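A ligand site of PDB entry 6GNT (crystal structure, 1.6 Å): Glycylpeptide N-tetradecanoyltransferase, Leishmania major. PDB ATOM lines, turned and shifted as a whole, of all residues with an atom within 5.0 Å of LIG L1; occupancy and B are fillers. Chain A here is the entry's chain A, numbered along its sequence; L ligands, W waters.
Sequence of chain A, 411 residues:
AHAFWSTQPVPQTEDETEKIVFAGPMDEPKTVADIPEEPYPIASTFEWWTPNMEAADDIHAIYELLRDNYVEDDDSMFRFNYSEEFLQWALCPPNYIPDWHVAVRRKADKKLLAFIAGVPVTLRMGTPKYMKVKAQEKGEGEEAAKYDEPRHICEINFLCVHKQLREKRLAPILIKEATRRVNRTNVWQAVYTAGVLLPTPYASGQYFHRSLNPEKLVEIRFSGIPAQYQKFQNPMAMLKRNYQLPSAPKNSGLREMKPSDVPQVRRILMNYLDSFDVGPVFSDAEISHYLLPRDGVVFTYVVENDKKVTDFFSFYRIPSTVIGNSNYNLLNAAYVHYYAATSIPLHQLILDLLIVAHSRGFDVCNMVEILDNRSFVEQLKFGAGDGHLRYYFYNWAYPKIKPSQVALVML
A nitrogen (N3) of LIG L1 lies within salt-bridge range of the chain-end carboxylate (O) of Leu 411 (3.7 Å).
The backbone NH (N) of Asp 386 lies within hydrogen-bond range of an oxygen (O2) of LIG L1, at 3.1 Å.
A nitrogen (N4) of LIG L1 is in hydrogen-bond range of the side-chain hydroxyl (OG) of Ser 320, at 2.8 Å.
O of Tyr 207 is in hydrogen-bond range of N of Gly 385, 2.8 Å away.
The side-chain amide nitrogen (ND2) of Asn 157 is in hydrogen-bond range of the chain-end carboxylate (O) of Leu 411, 2.7 Å away.
OH of Tyr 82 lies within hydrogen-bond range of OXT of Leu 411.
The backbone NH (N) of Phe 78 lies within hydrogen-bond range of the side-chain carboxylate (OD1) of Asp 73 (3.1 Å).
N of Tyr 207 sits at hydrogen-bond distance from O of Gly 387 (3.0 Å).
ND2 of Asn 366 is in hydrogen-bond range of OH of Tyr 335, at 3.0 Å.
The side-chain amide oxygen of Asn 157 is in hydrogen-bond range of the side-chain hydroxyl of Tyr 70 (3.4 Å).
OG1 of Thr 193 lies within hydrogen-bond range of SD of Met 410 (3.5 Å).
OH of Tyr 70 touches C25 of LIG L1, 3.9 Å away.
CG1 of Val 71 touches C22 of LIG L1, 3.7 Å away.
CB of Asp 73 touches C13 of LIG L1 (3.7 Å).
CB of Phe 78 touches N4 of LIG L1 (3.5 Å).
CZ of Phe 80 touches C15 of LIG L1, 3.6 Å away.
Asn 157 touches LIG L1.
Thr 193 touches LIG L1.
N of Gly 195 touches C23 of LIG L1 (3.9 Å).
Tyr 207 touches LIG L1 (CZ to C11, 3.5 Å).
CG of His 209 touches C8 of LIG L1, 3.7 Å away.
CD2 of Leu 331 touches C17 of LIG L1, 3.9 Å away.
Asn 366 touches LIG L1 (ND2 to C17, 3.6 Å).
CA of Gly 385 touches O2 of LIG L1, at 3.4 Å.
Gly 387 touches LIG L1.
Leu 389 touches LIG L1 (CD1 to C24, 3.7 Å).
CB of Met 410 touches C27 of LIG L1, at 3.7 Å.
Within 4 Å of LIG L1: Tyr 70, Val 71, Asp 73, Phe 78, Phe 80, Asn 157, Thr 193, Gly 195, Tyr 207, His 209, Ser 320, Leu 331, Asn 366, Gly 385, Asp 386, Gly 387, Leu 389, Met 410 and Leu 411.
The nearest printed residue that does not touch LIG L1 is Tyr 335 (4.05 Å).
Water W2 bridges O1 of LIG L1 (2.7 Å) and ND1 of His 209 (2.8 Å).
Water W3 lies within hydrogen-bond range of OD2 of Asp 73 (2.6 Å), N2 of LIG L1 (2.8 Å) and OD2 of Asp 386 (2.9 Å).
Water W1 lies within hydrogen-bond range of OH of Tyr 70 (2.7 Å), OD1 of Asn 157 (2.7 Å), OH of Tyr 82 (2.9 Å) and O of Leu 411 (3.1 Å).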
ATOM      1  N   TYR A  70      24.141 -21.099  -5.028  1.00  0.00           N
ATOM      2  CA  TYR A  70      23.927 -20.779  -6.455  1.00  0.00           C
ATOM      3  C   TYR A  70      25.224 -20.619  -7.169  1.00  0.00           C
ATOM      4  O   TYR A  70      26.307 -21.080  -6.719  1.00  0.00           O
ATOM      5  CB  TYR A  70      22.939 -19.621  -6.635  1.00  0.00           C
ATOM      6  CG  TYR A  70      22.262 -19.480  -8.045  1.00  0.00           C
ATOM      7  CD1 TYR A  70      21.708 -20.609  -8.638  1.00  0.00           C
ATOM      8  CD2 TYR A  70      22.254 -18.242  -8.732  1.00  0.00           C
ATOM      9  CE1 TYR A  70      21.105 -20.560  -9.907  1.00  0.00           C
ATOM     10  CE2 TYR A  70      21.634 -18.170 -10.018  1.00  0.00           C
ATOM     11  CZ  TYR A  70      21.061 -19.309 -10.536  1.00  0.00           C
ATOM     12  OH  TYR A  70      20.483 -19.122 -11.767  1.00  0.00           O
ATOM     13  N   VAL A  71      25.214 -20.006  -8.331  1.00  0.00           N
ATOM     14  CA  VAL A  71      26.323 -19.997  -9.282  1.00  0.00           C
ATOM     15  C   VAL A  71      27.551 -19.285  -8.756  1.00  0.00           C
ATOM     16  O   VAL A  71      27.448 -18.174  -8.243  1.00  0.00           O
ATOM     17  CB  VAL A  71      25.909 -19.323 -10.562  1.00  0.00           C
ATOM     18  CG1 VAL A  71      27.059 -19.301 -11.527  1.00  0.00           C
ATOM     19  CG2 VAL A  71      24.766 -20.162 -11.277  1.00  0.00           C
ATOM     20  N   GLU A  72      28.695 -19.981  -8.844  1.00  0.00           N
ATOM     21  CA  GLU A  72      30.074 -19.437  -8.661  1.00  0.00           C
ATOM     22  C   GLU A  72      30.822 -19.364  -9.928  1.00  0.00           C
ATOM     23  O   GLU A  72      30.506 -20.063 -10.907  1.00  0.00           O
ATOM     24  CB  GLU A  72      30.878 -20.335  -7.659  1.00  0.00           C
ATOM     25  CG  GLU A  72      30.144 -20.511  -6.387  1.00  0.00           C
ATOM     26  CD  GLU A  72      30.807 -21.407  -5.430  1.00  0.00           C
ATOM     27  OE1 GLU A  72      30.111 -21.700  -4.429  1.00  0.00           O
ATOM     28  OE2 GLU A  72      32.019 -21.799  -5.591  1.00  0.00           O
ATOM     29  N   ASP A  73      31.815 -18.499  -9.961  1.00  0.00           N
ATOM     30  CA  ASP A  73      32.694 -18.614 -11.149  1.00  0.00           C
ATOM     31  C   ASP A  73      33.663 -19.818 -11.046  1.00  0.00           C
ATOM     32  O   ASP A  73      33.580 -20.565 -10.094  1.00  0.00           O
ATOM     33  CB  ASP A  73      33.422 -17.351 -11.480  1.00  0.00           C
ATOM     34  CG  ASP A  73      34.342 -16.925 -10.379  1.00  0.00           C
ATOM     35  OD1 ASP A  73      34.180 -17.400  -9.220  1.00  0.00           O
ATOM     36  OD2 ASP A  73      35.190 -16.036 -10.696  1.00  0.00           O
ATOM     37  N   PHE A  78      33.650 -15.735  -6.688  1.00  0.00           N
ATOM     38  CA  PHE A  78      32.393 -14.989  -6.527  1.00  0.00           C
ATOM     39  C   PHE A  78      31.245 -15.975  -6.463  1.00  0.00           C
ATOM     40  O   PHE A  78      31.282 -16.960  -7.244  1.00  0.00           O
ATOM     41  CB  PHE A  78      32.158 -14.028  -7.711  1.00  0.00           C
ATOM     42  CG  PHE A  78      33.274 -12.972  -7.884  1.00  0.00           C
ATOM     43  CD1 PHE A  78      33.425 -11.949  -6.920  1.00  0.00           C
ATOM     44  CD2 PHE A  78      34.090 -12.973  -9.037  1.00  0.00           C
ATOM     45  CE1 PHE A  78      34.488 -10.910  -7.106  1.00  0.00           C
ATOM     46  CE2 PHE A  78      35.152 -12.023  -9.220  1.00  0.00           C
ATOM     47  CZ  PHE A  78      35.335 -10.993  -8.245  1.00  0.00           C
ATOM     48  N   ARG A  79      30.185 -15.671  -5.695  1.00  0.00           N
ATOM     49  CA  ARG A  79      28.945 -16.424  -5.893  1.00  0.00           C
ATOM     50  C   ARG A  79      27.798 -15.376  -5.935  1.00  0.00           C
ATOM     51  O   ARG A  79      27.730 -14.467  -5.128  1.00  0.00           O
ATOM     52  CB  ARG A  79      28.716 -17.357  -4.709  1.00  0.00           C
ATOM     53  CG  ARG A  79      27.433 -18.241  -4.766  1.00  0.00           C
ATOM     54  CD  ARG A  79      27.441 -19.468  -3.796  1.00  0.00           C
ATOM     55  NE  ARG A  79      27.666 -19.097  -2.431  1.00  0.00           N
ATOM     56  CZ  ARG A  79      28.758 -19.344  -1.705  1.00  0.00           C
ATOM     57  NH1 ARG A  79      29.776 -20.071  -2.182  1.00  0.00           N
ATOM     58  NH2 ARG A  79      28.763 -18.933  -0.449  1.00  0.00           N
ATOM     59  N   PHE A  80      26.865 -15.552  -6.859  1.00  0.00           N
ATOM     60  CA  PHE A  80      25.790 -14.519  -6.934  1.00  0.00           C
ATOM     61  C   PHE A  80      24.974 -14.496  -5.624  1.00  0.00           C
ATOM     62  O   PHE A  80      24.799 -15.520  -4.958  1.00  0.00           O
ATOM     63  CB  PHE A  80      24.814 -14.905  -8.060  1.00  0.00           C
ATOM     64  CG  PHE A  80      25.349 -14.704  -9.406  1.00  0.00           C
ATOM     65  CD1 PHE A  80      25.647 -13.461  -9.903  1.00  0.00           C
ATOM     66  CD2 PHE A  80      25.602 -15.815 -10.220  1.00  0.00           C
ATOM     67  CE1 PHE A  80      26.189 -13.299 -11.156  1.00  0.00           C
ATOM     68  CE2 PHE A  80      26.170 -15.640 -11.485  1.00  0.00           C
ATOM     69  CZ  PHE A  80      26.388 -14.350 -11.982  1.00  0.00           C
ATOM     70  N   TYR A  82      21.654 -12.805  -5.225  1.00  0.00           N
ATOM     71  CA  TYR A  82      20.399 -12.176  -5.581  1.00  0.00           C
ATOM     72  C   TYR A  82      19.650 -11.789  -4.324  1.00  0.00           C
ATOM     73  O   TYR A  82      19.484 -12.582  -3.378  1.00  0.00           O
ATOM     74  CB  TYR A  82      19.591 -13.151  -6.376  1.00  0.00           C
ATOM     75  CG  TYR A  82      20.039 -13.386  -7.790  1.00  0.00           C
ATOM     76  CD1 TYR A  82      19.588 -12.568  -8.831  1.00  0.00           C
ATOM     77  CD2 TYR A  82      20.941 -14.412  -8.117  1.00  0.00           C
ATOM     78  CE1 TYR A  82      19.932 -12.863 -10.185  1.00  0.00           C
ATOM     79  CE2 TYR A  82      21.314 -14.656  -9.443  1.00  0.00           C
ATOM     80  CZ  TYR A  82      20.750 -13.900 -10.466  1.00  0.00           C
ATOM     81  OH  TYR A  82      21.113 -14.063 -11.779  1.00  0.00           O
ATOM     82  N   ASN A 157      14.945 -20.485 -14.865  1.00  0.00           N
ATOM     83  CA  ASN A 157      16.097 -19.850 -14.191  1.00  0.00           C
ATOM     84  C   ASN A 157      16.165 -20.346 -12.758  1.00  0.00           C
ATOM     85  O   ASN A 157      15.259 -21.018 -12.261  1.00  0.00           O
ATOM     86  CB  ASN A 157      15.769 -18.301 -14.211  1.00  0.00           C
ATOM     87  CG  ASN A 157      16.946 -17.378 -14.112  1.00  0.00           C
ATOM     88  OD1 ASN A 157      18.022 -17.756 -13.760  1.00  0.00           O
ATOM     89  ND2 ASN A 157      16.710 -16.058 -14.348  1.00  0.00           N
ATOM     90  N   THR A 193      19.341 -20.203 -20.161  1.00  0.00           N
ATOM     91  CA  THR A 193      20.763 -19.946 -20.336  1.00  0.00           C
ATOM     92  C   THR A 193      21.528 -20.659 -19.201  1.00  0.00           C
ATOM     93  O   THR A 193      20.970 -20.937 -18.106  1.00  0.00           O
ATOM     94  CB  THR A 193      21.066 -18.495 -20.355  1.00  0.00           C
ATOM     95  OG1 THR A 193      20.631 -17.884 -19.130  1.00  0.00           O
ATOM     96  CG2 THR A 193      20.444 -17.799 -21.561  1.00  0.00           C
ATOM     97  N   ALA A 194      22.821 -20.937 -19.494  1.00  0.00           N
ATOM     98  CA  ALA A 194      23.713 -21.507 -18.446  1.00  0.00           C
ATOM     99  C   ALA A 194      25.118 -21.066 -18.770  1.00  0.00           C
ATOM    100  O   ALA A 194      25.440 -20.776 -19.946  1.00  0.00           O
ATOM    101  CB  ALA A 194      23.605 -23.009 -18.398  1.00  0.00           C
ATOM    102  N   GLY A 195      25.961 -21.071 -17.785  1.00  0.00           N
ATOM    103  CA  GLY A 195      27.396 -20.793 -18.005  1.00  0.00           C
ATOM    104  C   GLY A 195      28.126 -22.051 -18.309  1.00  0.00           C
ATOM    105  O   GLY A 195      29.352 -21.970 -18.410  1.00  0.00           O
ATOM    106  N   TYR A 207      31.100 -12.863 -21.386  1.00  0.00           N
ATOM    107  CA  TYR A 207      30.807 -11.769 -20.468  1.00  0.00           C
ATOM    108  C   TYR A 207      31.829 -10.677 -20.610  1.00  0.00           C
ATOM    109  O   TYR A 207      32.952 -10.939 -20.947  1.00  0.00           O
ATOM    110  CB  TYR A 207      30.827 -12.240 -19.022  1.00  0.00           C
ATOM    111  CG  TYR A 207      29.489 -12.810 -18.552  1.00  0.00           C
ATOM    112  CD1 TYR A 207      28.558 -12.016 -17.859  1.00  0.00           C
ATOM    113  CD2 TYR A 207      29.178 -14.115 -18.801  1.00  0.00           C
ATOM    114  CE1 TYR A 207      27.345 -12.570 -17.414  1.00  0.00           C
ATOM    115  CE2 TYR A 207      27.986 -14.701 -18.326  1.00  0.00           C
ATOM    116  CZ  TYR A 207      27.084 -13.900 -17.697  1.00  0.00           C
ATOM    117  OH  TYR A 207      25.835 -14.400 -17.320  1.00  0.00           O
ATOM    118  N   HIS A 209      33.038  -6.791 -18.560  1.00  0.00           N
ATOM    119  CA  HIS A 209      32.818  -5.989 -17.331  1.00  0.00           C
ATOM    120  C   HIS A 209      33.534  -4.682 -17.466  1.00  0.00           C
ATOM    121  O   HIS A 209      34.539  -4.620 -18.182  1.00  0.00           O
ATOM    122  CB  HIS A 209      33.329  -6.708 -16.067  1.00  0.00           C
ATOM    123  CG  HIS A 209      34.718  -7.187 -16.212  1.00  0.00           C
ATOM    124  ND1 HIS A 209      35.049  -8.496 -16.512  1.00  0.00           N
ATOM    125  CD2 HIS A 209      35.888  -6.503 -16.158  1.00  0.00           C
ATOM    126  CE1 HIS A 209      36.372  -8.588 -16.588  1.00  0.00           C
ATOM    127  NE2 HIS A 209      36.896  -7.388 -16.414  1.00  0.00           N
ATOM    128  N   LEU A 217      37.924  -3.458  -6.884  1.00  0.00           N
ATOM    129  CA  LEU A 217      38.131  -4.537  -7.865  1.00  0.00           C
ATOM    130  C   LEU A 217      39.509  -5.189  -7.982  1.00  0.00           C
ATOM    131  O   LEU A 217      39.623  -6.425  -8.094  1.00  0.00           O
ATOM    132  CB  LEU A 217      37.732  -4.023  -9.227  1.00  0.00           C
ATOM    133  CG  LEU A 217      36.244  -4.094  -9.443  1.00  0.00           C
ATOM    134  CD1 LEU A 217      35.890  -3.417 -10.749  1.00  0.00           C
ATOM    135  CD2 LEU A 217      35.877  -5.580  -9.483  1.00  0.00           C
ATOM    136  N   SER A 320      27.398  -9.923  -5.598  1.00  0.00           N
ATOM    137  CA  SER A 320      28.016 -11.287  -5.467  1.00  0.00           C
ATOM    138  C   SER A 320      28.804 -11.323  -4.181  1.00  0.00           C
ATOM    139  O   SER A 320      29.498 -10.362  -3.851  1.00  0.00           O
ATOM    140  CB  SER A 320      28.930 -11.581  -6.614  1.00  0.00           C
ATOM    141  OG  SER A 320      28.131 -11.939  -7.760  1.00  0.00           O
ATOM    142  N   LEU A 331      30.506  -7.692  -3.724  1.00  0.00           N
ATOM    143  CA  LEU A 331      30.810  -6.903  -4.921  1.00  0.00           C
ATOM    144  C   LEU A 331      29.434  -6.450  -5.475  1.00  0.00           C
ATOM    145  O   LEU A 331      28.522  -7.254  -5.630  1.00  0.00           O
ATOM    146  CB  LEU A 331      31.540  -7.721  -6.011  1.00  0.00           C
ATOM    147  CG  LEU A 331      32.048  -6.934  -7.234  1.00  0.00           C
ATOM    148  CD1 LEU A 331      33.041  -5.860  -6.965  1.00  0.00           C
ATOM    149  CD2 LEU A 331      32.695  -7.925  -8.167  1.00  0.00           C
ATOM    150  N   TYR A 335      24.152  -4.774 -14.017  1.00  0.00           N
ATOM    151  CA  TYR A 335      24.119  -5.559 -15.271  1.00  0.00           C
ATOM    152  C   TYR A 335      23.291  -4.760 -16.249  1.00  0.00           C
ATOM    153  O   TYR A 335      22.163  -4.309 -16.011  1.00  0.00           O
ATOM    154  CB  TYR A 335      23.386  -6.924 -14.987  1.00  0.00           C
ATOM    155  CG  TYR A 335      24.288  -7.843 -14.253  1.00  0.00           C
ATOM    156  CD1 TYR A 335      24.940  -8.800 -14.882  1.00  0.00           C
ATOM    157  CD2 TYR A 335      24.519  -7.654 -12.849  1.00  0.00           C
ATOM    158  CE1 TYR A 335      25.870  -9.634 -14.189  1.00  0.00           C
ATOM    159  CE2 TYR A 335      25.454  -8.439 -12.167  1.00  0.00           C
ATOM    160  CZ  TYR A 335      26.115  -9.420 -12.821  1.00  0.00           C
ATOM    161  OH  TYR A 335      27.080 -10.201 -12.136  1.00  0.00           O
ATOM    162  N   VAL A 364      31.163  -2.329 -10.425  1.00  0.00           N
ATOM    163  CA  VAL A 364      31.469  -2.856 -11.742  1.00  0.00           C
ATOM    164  C   VAL A 364      30.128  -2.901 -12.489  1.00  0.00           C
ATOM    165  O   VAL A 364      29.037  -3.091 -11.889  1.00  0.00           O
ATOM    166  CB  VAL A 364      32.171  -4.247 -11.621  1.00  0.00           C
ATOM    167  CG1 VAL A 364      31.177  -5.289 -11.041  1.00  0.00           C
ATOM    168  CG2 VAL A 364      32.640  -4.780 -12.985  1.00  0.00           C
ATOM    169  N   ASN A 366      28.465  -5.210 -15.678  1.00  0.00           N
ATOM    170  CA  ASN A 366      28.688  -6.482 -16.354  1.00  0.00           C
ATOM    171  C   ASN A 366      27.648  -6.632 -17.427  1.00  0.00           C
ATOM    172  O   ASN A 366      26.501  -6.060 -17.344  1.00  0.00           O
ATOM    173  CB  ASN A 366      28.519  -7.711 -15.396  1.00  0.00           C
ATOM    174  CG  ASN A 366      29.646  -7.860 -14.365  1.00  0.00           C
ATOM    175  OD1 ASN A 366      30.733  -7.310 -14.503  1.00  0.00           O
ATOM    176  ND2 ASN A 366      29.368  -8.642 -13.309  1.00  0.00           N
ATOM    177  N   GLY A 385      35.352 -11.044 -19.494  1.00  0.00           N
ATOM    178  CA  GLY A 385      35.465 -11.814 -18.226  1.00  0.00           C
ATOM    179  C   GLY A 385      35.830 -13.267 -18.652  1.00  0.00           C
ATOM    180  O   GLY A 385      36.083 -13.591 -19.829  1.00  0.00           O
ATOM    181  N   ASP A 386      35.757 -14.128 -17.645  1.00  0.00           N
ATOM    182  CA  ASP A 386      36.109 -15.542 -17.907  1.00  0.00           C
ATOM    183  C   ASP A 386      34.887 -16.374 -18.175  1.00  0.00           C
ATOM    184  O   ASP A 386      34.985 -17.542 -18.521  1.00  0.00           O
ATOM    185  CB  ASP A 386      37.070 -16.113 -16.875  1.00  0.00           C
ATOM    186  CG  ASP A 386      36.452 -16.318 -15.542  1.00  0.00           C
ATOM    187  OD1 ASP A 386      37.242 -16.697 -14.570  1.00  0.00           O
ATOM    188  OD2 ASP A 386      35.209 -16.079 -15.378  1.00  0.00           O
ATOM    189  N   GLY A 387      33.730 -15.786 -18.107  1.00  0.00           N
ATOM    190  CA  GLY A 387      32.481 -16.523 -18.341  1.00  0.00           C
ATOM    191  C   GLY A 387      31.954 -16.427 -19.758  1.00  0.00           C
ATOM    192  O   GLY A 387      32.270 -15.488 -20.533  1.00  0.00           O
ATOM    193  N   LEU A 389      28.032 -17.151 -21.553  1.00  0.00           N
ATOM    194  CA  LEU A 389      26.640 -17.477 -21.367  1.00  0.00           C
ATOM    195  C   LEU A 389      26.114 -18.204 -22.594  1.00  0.00           C
ATOM    196  O   LEU A 389      26.287 -17.685 -23.740  1.00  0.00           O
ATOM    197  CB  LEU A 389      25.826 -16.223 -21.175  1.00  0.00           C
ATOM    198  CG  LEU A 389      24.407 -16.478 -20.703  1.00  0.00           C
ATOM    199  CD1 LEU A 389      24.385 -17.259 -19.321  1.00  0.00           C
ATOM    200  CD2 LEU A 389      23.623 -15.289 -20.568  1.00  0.00           C
ATOM    201  N   MET A 410      18.537 -12.453 -19.785  1.00  0.00           N
ATOM    202  CA  MET A 410      18.012 -13.292 -18.692  1.00  0.00           C
ATOM    203  C   MET A 410      18.655 -12.812 -17.381  1.00  0.00           C
ATOM    204  O   MET A 410      19.864 -12.493 -17.355  1.00  0.00           O
ATOM    205  CB  MET A 410      18.320 -14.776 -18.892  1.00  0.00           C
ATOM    206  CG  MET A 410      17.486 -15.347 -20.110  1.00  0.00           C
ATOM    207  SD  MET A 410      17.301 -17.083 -19.849  1.00  0.00           S
ATOM    208  CE  MET A 410      16.418 -17.089 -18.323  1.00  0.00           C
ATOM    209  N   LEU A 411      17.814 -12.728 -16.377  1.00  0.00           N
ATOM    210  CA  LEU A 411      18.211 -12.130 -15.068  1.00  0.00           C
ATOM    211  C   LEU A 411      19.019 -13.138 -14.232  1.00  0.00           C
ATOM    212  O   LEU A 411      18.814 -14.359 -14.186  1.00  0.00           O
ATOM    213  CB  LEU A 411      16.915 -11.792 -14.324  1.00  0.00           C
ATOM    214  CG  LEU A 411      16.058 -10.754 -15.094  1.00  0.00           C
ATOM    215  CD1 LEU A 411      14.733 -10.480 -14.372  1.00  0.00           C
ATOM    216  CD2 LEU A 411      16.789  -9.462 -15.348  1.00  0.00           C
ATOM    217  OXT LEU A 411      19.940 -12.621 -13.543  1.00  0.00           O
HETATM  218  C1  LIG L   1      31.210 -13.092 -11.489  1.00  0.00           C
HETATM  219  C2  LIG L   1      29.421 -16.351 -15.125  1.00  0.00           C
HETATM  220  C3  LIG L   1      32.188 -12.338 -12.180  1.00  0.00           C
HETATM  221  C4  LIG L   1      32.288 -10.978 -11.904  1.00  0.00           C
HETATM  222  C5  LIG L   1      31.231 -14.161 -15.015  1.00  0.00           C
HETATM  223  C6  LIG L   1      34.591 -10.765 -12.789  1.00  0.00           C
HETATM  224  C7  LIG L   1      35.608  -9.584 -12.680  1.00  0.00           C
HETATM  225  C8  LIG L   1      34.712  -8.325 -12.657  1.00  0.00           C
HETATM  226  C9  LIG L   1      33.408  -8.776 -12.045  1.00  0.00           C
HETATM  227  C10 LIG L   1      29.844 -13.958 -15.034  1.00  0.00           C
HETATM  228  C11 LIG L   1      28.963 -15.028 -15.000  1.00  0.00           C
HETATM  229  N1  LIG L   1      33.246 -10.161 -12.528  1.00  0.00           N
HETATM  230  N2  LIG L   1      32.940 -12.910 -13.286  1.00  0.00           N
HETATM  231  C12 LIG L   1      30.397 -12.467 -10.489  1.00  0.00           C
HETATM  232  N3  LIG L   1      21.247 -16.863 -15.514  1.00  0.00           N
HETATM  233  O1  LIG L   1      31.577 -11.738 -15.162  1.00  0.00           O
HETATM  234  S1  LIG L   1      32.325 -12.962 -14.854  1.00  0.00           S
HETATM  235  O2  LIG L   1      33.488 -13.130 -15.779  1.00  0.00           O
HETATM  236  C13 LIG L   1      31.006 -14.496 -11.678  1.00  0.00           C
HETATM  237  C14 LIG L   1      30.126 -15.195 -10.944  1.00  0.00           C
HETATM  238  C15 LIG L   1      29.340 -14.532  -9.989  1.00  0.00           C
HETATM  239  N4  LIG L   1      29.523 -13.182  -9.795  1.00  0.00           N
HETATM  240  C16 LIG L   1      30.531 -11.100 -10.224  1.00  0.00           C
HETATM  241  C17 LIG L   1      31.455 -10.364 -10.929  1.00  0.00           C
HETATM  242  C18 LIG L   1      31.714 -15.500 -15.029  1.00  0.00           C
HETATM  243  C19 LIG L   1      30.792 -16.539 -15.086  1.00  0.00           C
HETATM  244  C20 LIG L   1      28.554 -17.666 -15.238  1.00  0.00           C
HETATM  245  C21 LIG L   1      27.131 -17.546 -15.756  1.00  0.00           C
HETATM  246  C22 LIG L   1      26.115 -17.489 -14.655  1.00  0.00           C
HETATM  247  C23 LIG L   1      25.105 -18.533 -14.999  1.00  0.00           C
HETATM  248  C24 LIG L   1      23.882 -18.093 -15.772  1.00  0.00           C
HETATM  249  C25 LIG L   1      22.790 -18.593 -14.836  1.00  0.00           C
HETATM  250  C26 LIG L   1      21.457 -18.340 -15.540  1.00  0.00           C
HETATM  251  C27 LIG L   1      19.916 -16.679 -16.202  1.00  0.00           C
HETATM  252  C28 LIG L   1      22.335 -16.036 -16.018  1.00  0.00           C
HETATM  253  C29 LIG L   1      23.697 -16.589 -15.641  1.00  0.00           C
HETATM  254  S1  LG2 L   2      21.742 -22.341 -15.091  1.00  0.00           S
HETATM  255  C1  LG2 L   2      22.317 -22.146 -13.362  1.00  0.00           C
HETATM  256  C2  LG2 L   2      22.312 -23.548 -12.782  1.00  0.00           C
HETATM  257  N1  LG2 L   2      22.684 -23.451 -11.330  1.00  0.00           N
HETATM  258  C3  LG2 L   2      23.905 -23.524 -10.904  1.00  0.00           C
HETATM  259  O1  LG2 L   2      24.971 -23.671 -11.561  1.00  0.00           O
HETATM  260  C4  LG2 L   2      24.018 -23.373  -9.379  1.00  0.00           C
HETATM  261  C5  LG2 L   2      25.150 -24.244  -8.720  1.00  0.00           C
HETATM  262  N2  LG2 L   2      25.081 -25.632  -9.113  1.00  0.00           N
HETATM  263  C6  LG2 L   2      24.053 -26.415  -8.763  1.00  0.00           C
HETATM  264  O2  LG2 L   2      23.133 -26.041  -8.056  1.00  0.00           O
HETATM  265  C7  LG2 L   2      24.074 -27.801  -9.300  1.00  0.00           C
HETATM  266  O3  LG2 L   2      25.395 -28.195  -9.586  1.00  0.00           O
HETATM  267  C8  LG2 L   2      23.094 -28.104 -10.448  1.00  0.00           C
HETATM  268  C9  LG2 L   2      23.336 -29.548 -10.903  1.00  0.00           C
HETATM  269  C10 LG2 L   2      23.343 -27.151 -11.644  1.00  0.00           C
HETATM  270  C11 LG2 L   2      21.635 -27.917 -10.024  1.00  0.00           C
HETATM  271  N3  LG2 L   2      21.399 -27.041 -16.442  1.00  0.00           N
HETATM  272  O4  LG2 L   2      21.745 -33.542  -9.749  1.00  0.00           O
HETATM  273  P1  LG2 L   2      22.904 -33.831 -10.557  1.00  0.00           P
HETATM  274  C12 LG2 L   2      22.996 -31.871 -15.692  1.00  0.00           C
HETATM  275  C13 LG2 L   2      20.822 -28.170 -16.854  1.00  0.00           C
HETATM  276  O5  LG2 L   2      23.686 -35.158 -10.282  1.00  0.00           O
HETATM  277  P2  LG2 L   2      24.204 -31.516  -9.516  1.00  0.00           P
HETATM  278  C14 LG2 L   2      20.045 -22.379 -14.928  1.00  0.00           C
HETATM  279  O6  LG2 L   2      19.460 -22.082 -13.894  1.00  0.00           O
HETATM  280  C15 LG2 L   2      24.302 -32.637 -15.955  1.00  0.00           C
HETATM  281  O7  LG2 L   2      24.763 -32.455 -17.276  1.00  0.00           O
HETATM  282  N4  LG2 L   2      21.406 -29.358 -16.598  1.00  0.00           N
HETATM  283  O8  LG2 L   2      24.046 -32.654 -10.597  1.00  0.00           O
HETATM  284  C16 LG2 L   2      19.174 -22.894 -16.093  1.00  0.00           C
HETATM  285  C17 LG2 L   2      23.739 -34.032 -15.622  1.00  0.00           C
HETATM  286  O9  LG2 L   2      22.966 -34.561 -16.705  1.00  0.00           O
HETATM  287  P3  LG2 L   2      23.632 -35.657 -17.677  1.00  0.00           P
HETATM  288  C18 LG2 L   2      22.551 -29.382 -15.876  1.00  0.00           C
HETATM  289  O10 LG2 L   2      25.553 -30.958  -9.840  1.00  0.00           O
HETATM  290  C19 LG2 L   2      18.726 -24.305 -15.825  1.00  0.00           C
HETATM  291  C20 LG2 L   2      22.803 -33.855 -14.500  1.00  0.00           C
HETATM  292  O11 LG2 L   2      22.516 -32.405 -14.489  1.00  0.00           O
HETATM  293  C21 LG2 L   2      23.172 -28.216 -15.435  1.00  0.00           C
HETATM  294  O12 LG2 L   2      23.839 -31.967  -8.198  1.00  0.00           O
HETATM  295  C22 LG2 L   2      18.181 -24.958 -17.110  1.00  0.00           C
HETATM  296  C23 LG2 L   2      23.483 -34.054 -13.200  1.00  0.00           C
HETATM  297  O13 LG2 L   2      22.585 -33.898 -12.100  1.00  0.00           O
HETATM  298  C24 LG2 L   2      22.543 -26.978 -15.733  1.00  0.00           C
HETATM  299  N5  LG2 L   2      22.969 -25.745 -15.416  1.00  0.00           N
HETATM  300  O14 LG2 L   2      23.036 -30.404  -9.878  1.00  0.00           O
HETATM  301  C25 LG2 L   2      17.636 -26.336 -16.699  1.00  0.00           C
HETATM  302  N6  LG2 L   2      24.267 -28.555 -14.751  1.00  0.00           N
HETATM  303  O15 LG2 L   2      24.907 -34.996 -18.269  1.00  0.00           O
HETATM  304  C26 LG2 L   2      17.010 -27.077 -17.886  1.00  0.00           C
HETATM  305  C27 LG2 L   2      24.349 -29.874 -14.777  1.00  0.00           C
HETATM  306  O16 LG2 L   2      23.952 -36.897 -16.798  1.00  0.00           O
HETATM  307  C28 LG2 L   2      15.585 -26.559 -18.123  1.00  0.00           C
HETATM  308  N7  LG2 L   2      23.315 -30.422 -15.448  1.00  0.00           N
HETATM  309  O17 LG2 L   2      22.719 -35.906 -18.852  1.00  0.00           O
HETATM  310  C29 LG2 L   2      14.969 -27.363 -19.297  1.00  0.00           C
HETATM  311  C30 LG2 L   2      13.568 -26.858 -19.712  1.00  0.00           C
HETATM  312  C31 LG2 L   2      12.555 -27.259 -18.692  1.00  0.00           C
HETATM  313  C32 LG2 L   2      11.117 -26.762 -18.983  1.00  0.00           C
HETATM  314  C33 LG2 L   2      10.534 -27.398 -20.278  1.00  0.00           C
HETATM  315  C34 LG2 L   2       9.059 -26.850 -20.449  1.00  0.00           C
HETATM  316  C35 LG2 L   2       8.530 -27.264 -21.869  1.00  0.00           C
HETATM  317  O   HOH W   1      20.331 -16.667 -12.759  1.00  0.00           O
HETATM  318  O   HOH W   2      32.648  -9.919 -16.848  1.00  0.00           O
HETATM  319  O   HOH W   3      35.092 -14.600 -12.834  1.00  0.00           O
